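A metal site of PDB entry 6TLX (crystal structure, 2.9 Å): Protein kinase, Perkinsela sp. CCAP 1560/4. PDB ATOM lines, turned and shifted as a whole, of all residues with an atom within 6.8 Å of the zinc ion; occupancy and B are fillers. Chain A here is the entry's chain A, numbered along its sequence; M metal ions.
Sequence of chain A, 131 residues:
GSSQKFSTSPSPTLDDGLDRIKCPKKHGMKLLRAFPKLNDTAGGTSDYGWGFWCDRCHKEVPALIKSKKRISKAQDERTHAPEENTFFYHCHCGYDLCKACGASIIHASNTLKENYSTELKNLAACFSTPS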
ATOM      1  N   CYS A  54     -15.835  19.780 -13.577  1.00  0.00           N
ATOM      2  CA  CYS A  54     -14.608  18.974 -13.647  1.00  0.00           C
ATOM      3  C   CYS A  54     -13.525  19.691 -12.825  1.00  0.00           C
ATOM      4  O   CYS A  54     -13.340  20.895 -12.973  1.00  0.00           O
ATOM      5  CB  CYS A  54     -14.170  18.720 -15.091  1.00  0.00           C
ATOM      6  SG  CYS A  54     -12.570  17.869 -15.229  1.00  0.00           S
ATOM      7  N   ASP A  55     -12.857  18.957 -11.960  1.00  0.00           N
ATOM      8  CA  ASP A  55     -11.812  19.607 -11.162  1.00  0.00           C
ATOM      9  C   ASP A  55     -10.624  19.890 -12.060  1.00  0.00           C
ATOM     10  O   ASP A  55      -9.656  20.424 -11.572  1.00  0.00           O
ATOM     11  CB  ASP A  55     -11.313  18.677 -10.065  1.00  0.00           C
ATOM     12  CG  ASP A  55     -12.176  18.687  -8.836  1.00  0.00           C
ATOM     13  OD1 ASP A  55     -13.209  19.287  -8.862  1.00  0.00           O
ATOM     14  OD2 ASP A  55     -11.780  18.079  -7.875  1.00  0.00           O
ATOM     15  N   ARG A  56     -10.685  19.544 -13.334  1.00  0.00           N
ATOM     16  CA  ARG A  56      -9.476  19.805 -14.125  1.00  0.00           C
ATOM     17  C   ARG A  56      -9.770  20.770 -15.249  1.00  0.00           C
ATOM     18  O   ARG A  56      -9.083  21.725 -15.342  1.00  0.00           O
ATOM     19  CB  ARG A  56      -8.884  18.519 -14.643  1.00  0.00           C
ATOM     20  CG  ARG A  56      -7.792  18.757 -15.668  1.00  0.00           C
ATOM     21  CD  ARG A  56      -6.666  17.755 -15.664  1.00  0.00           C
ATOM     22  NE  ARG A  56      -6.010  17.811 -16.950  1.00  0.00           N
ATOM     23  CZ  ARG A  56      -6.652  17.577 -18.066  1.00  0.00           C
ATOM     24  NH1 ARG A  56      -6.015  17.642 -19.214  1.00  0.00           N
ATOM     25  NH2 ARG A  56      -7.931  17.280 -18.035  1.00  0.00           N
ATOM     26  N   CYS A  57     -10.780  20.515 -16.052  1.00  0.00           N
ATOM     27  CA  CYS A  57     -11.015  21.457 -17.145  1.00  0.00           C
ATOM     28  C   CYS A  57     -12.151  22.383 -16.741  1.00  0.00           C
ATOM     29  O   CYS A  57     -12.635  23.056 -17.569  1.00  0.00           O
ATOM     30  CB  CYS A  57     -11.414  20.705 -18.391  1.00  0.00           C
ATOM     31  SG  CYS A  57     -13.045  20.023 -18.212  1.00  0.00           S
ATOM     32  N   HIS A  58     -12.566  22.344 -15.497  1.00  0.00           N
ATOM     33  CA  HIS A  58     -13.594  23.253 -14.968  1.00  0.00           C
ATOM     34  C   HIS A  58     -14.937  23.176 -15.700  1.00  0.00           C
ATOM     35  O   HIS A  58     -15.869  23.841 -15.264  1.00  0.00           O
ATOM     36  CB  HIS A  58     -13.112  24.703 -14.858  1.00  0.00           C
ATOM     37  CG  HIS A  58     -11.830  24.828 -14.111  1.00  0.00           C
ATOM     38  ND1 HIS A  58     -11.643  24.169 -12.915  1.00  0.00           N
ATOM     39  CD2 HIS A  58     -10.699  25.479 -14.447  1.00  0.00           C
ATOM     40  CE1 HIS A  58     -10.400  24.451 -12.534  1.00  0.00           C
ATOM     41  NE2 HIS A  58      -9.781  25.229 -13.426  1.00  0.00           N
ATOM     42  N   LYS A  59     -15.078  22.335 -16.748  1.00  0.00           N
ATOM     43  CA  LYS A  59     -16.365  22.222 -17.455  1.00  0.00           C
ATOM     44  C   LYS A  59     -17.543  21.930 -16.561  1.00  0.00           C
ATOM     45  O   LYS A  59     -17.472  21.021 -15.727  1.00  0.00           O
ATOM     46  CB  LYS A  59     -16.331  21.187 -18.600  1.00  0.00           C
ATOM     47  N   VAL A  61     -20.661  20.139 -16.209  1.00  0.00           N
ATOM     48  CA  VAL A  61     -21.432  19.048 -16.809  1.00  0.00           C
ATOM     49  C   VAL A  61     -22.689  18.960 -15.976  1.00  0.00           C
ATOM     50  O   VAL A  61     -22.638  18.493 -14.834  1.00  0.00           O
ATOM     51  CB  VAL A  61     -20.677  17.703 -16.777  1.00  0.00           C
ATOM     52  CG1 VAL A  61     -21.539  16.594 -17.350  1.00  0.00           C
ATOM     53  CG2 VAL A  61     -19.345  17.787 -17.502  1.00  0.00           C
ATOM     54  N   ASP A  96     -13.522  15.230  -9.143  1.00  0.00           N
ATOM     55  CA  ASP A  96     -14.250  14.665 -10.297  1.00  0.00           C
ATOM     56  C   ASP A  96     -13.599  15.015 -11.628  1.00  0.00           C
ATOM     57  O   ASP A  96     -12.987  16.066 -11.781  1.00  0.00           O
ATOM     58  CB  ASP A  96     -15.688  15.163 -10.373  1.00  0.00           C
ATOM     59  CG  ASP A  96     -16.508  14.835  -9.159  1.00  0.00           C
ATOM     60  OD1 ASP A  96     -16.248  13.807  -8.534  1.00  0.00           O
ATOM     61  OD2 ASP A  96     -17.409  15.611  -8.843  1.00  0.00           O
ATOM     62  N   LEU A  97     -13.795  14.133 -12.624  1.00  0.00           N
ATOM     63  CA  LEU A  97     -13.299  14.385 -13.959  1.00  0.00           C
ATOM     64  C   LEU A  97     -14.392  14.117 -14.959  1.00  0.00           C
ATOM     65  O   LEU A  97     -15.027  13.069 -14.901  1.00  0.00           O
ATOM     66  CB  LEU A  97     -12.104  13.504 -14.258  1.00  0.00           C
ATOM     67  CG  LEU A  97     -10.829  13.904 -13.543  1.00  0.00           C
ATOM     68  CD1 LEU A  97      -9.835  12.787 -13.551  1.00  0.00           C
ATOM     69  CD2 LEU A  97     -10.253  15.130 -14.147  1.00  0.00           C
ATOM     70  N   CYS A  98     -14.604  15.052 -15.869  1.00  0.00           N
ATOM     71  CA  CYS A  98     -15.522  14.893 -16.990  1.00  0.00           C
ATOM     72  C   CYS A  98     -14.997  13.778 -17.928  1.00  0.00           C
ATOM     73  O   CYS A  98     -13.812  13.421 -17.874  1.00  0.00           O
ATOM     74  CB  CYS A  98     -15.673  16.208 -17.753  1.00  0.00           C
ATOM     75  SG  CYS A  98     -14.160  16.749 -18.605  1.00  0.00           S
ATOM     76  N   LYS A  99     -15.814  13.321 -18.843  1.00  0.00           N
ATOM     77  CA  LYS A  99     -15.363  12.231 -19.729  1.00  0.00           C
ATOM     78  C   LYS A  99     -14.171  12.681 -20.556  1.00  0.00           C
ATOM     79  O   LYS A  99     -13.209  11.964 -20.663  1.00  0.00           O
ATOM     80  CB  LYS A  99     -16.515  11.981 -20.693  1.00  0.00           C
ATOM     81  CG  LYS A  99     -16.460  10.687 -21.467  1.00  0.00           C
ATOM     82  CD  LYS A  99     -17.764  10.441 -22.148  1.00  0.00           C
ATOM     83  CE  LYS A  99     -17.682   9.512 -23.331  1.00  0.00           C
ATOM     84  NZ  LYS A  99     -18.916   9.627 -24.133  1.00  0.00           N
ATOM     85  N   ALA A 100     -14.247  13.898 -21.047  1.00  0.00           N
ATOM     86  CA  ALA A 100     -13.204  14.444 -21.901  1.00  0.00           C
ATOM     87  C   ALA A 100     -11.839  14.363 -21.264  1.00  0.00           C
ATOM     88  O   ALA A 100     -10.884  13.956 -21.923  1.00  0.00           O
ATOM     89  CB  ALA A 100     -13.530  15.874 -22.276  1.00  0.00           C
ATOM     90  N   CYS A 101     -11.731  14.724 -19.977  1.00  0.00           N
ATOM     91  CA  CYS A 101     -10.460  14.681 -19.240  1.00  0.00           C
ATOM     92  C   CYS A 101     -10.007  13.229 -19.043  1.00  0.00           C
ATOM     93  O   CYS A 101      -8.825  12.930 -19.129  1.00  0.00           O
ATOM     94  CB  CYS A 101     -10.580  15.424 -17.913  1.00  0.00           C
ATOM     95  SG  CYS A 101     -10.561  17.230 -18.047  1.00  0.00           S
ATOM     96  N   GLY A 102     -10.953  12.332 -18.816  1.00  0.00           N
ATOM     97  CA  GLY A 102     -10.659  10.913 -18.678  1.00  0.00           C
ATOM     98  C   GLY A 102     -10.110  10.381 -19.991  1.00  0.00           C
ATOM     99  O   GLY A 102      -9.061   9.736 -20.029  1.00  0.00           O
HETATM  100 ZN    ZN M   1     -12.619  17.979 -17.710  1.00  0.00          ZN
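The side-chain sulfur of Cys 54 sits close to the backbone NH of Arg 56 (3.2 Å). SG of Cys 98 sits close to N of Ala 100 (3.8 Å). SG of Cys 101 sits close to NH2 of Arg 56, at 2.6 Å. SG of Cys 57 lies close to N of Lys 59 (3.4 Å). The backbone NH (N) of Cys 54 lies within hydrogen-bond range of the backbone carbonyl oxygen (O) of Lys 59 (3.0 Å).
Of the 14 residues printed, 4 come within 4 Å of the zinc ion.
The zinc ion is bound by SG of Cys 57 (2.1 Å), SG of Cys 98 (2.2 Å), SG of Cys 101 (2.2 Å) and SG of Cys 54 (2.5 Å).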
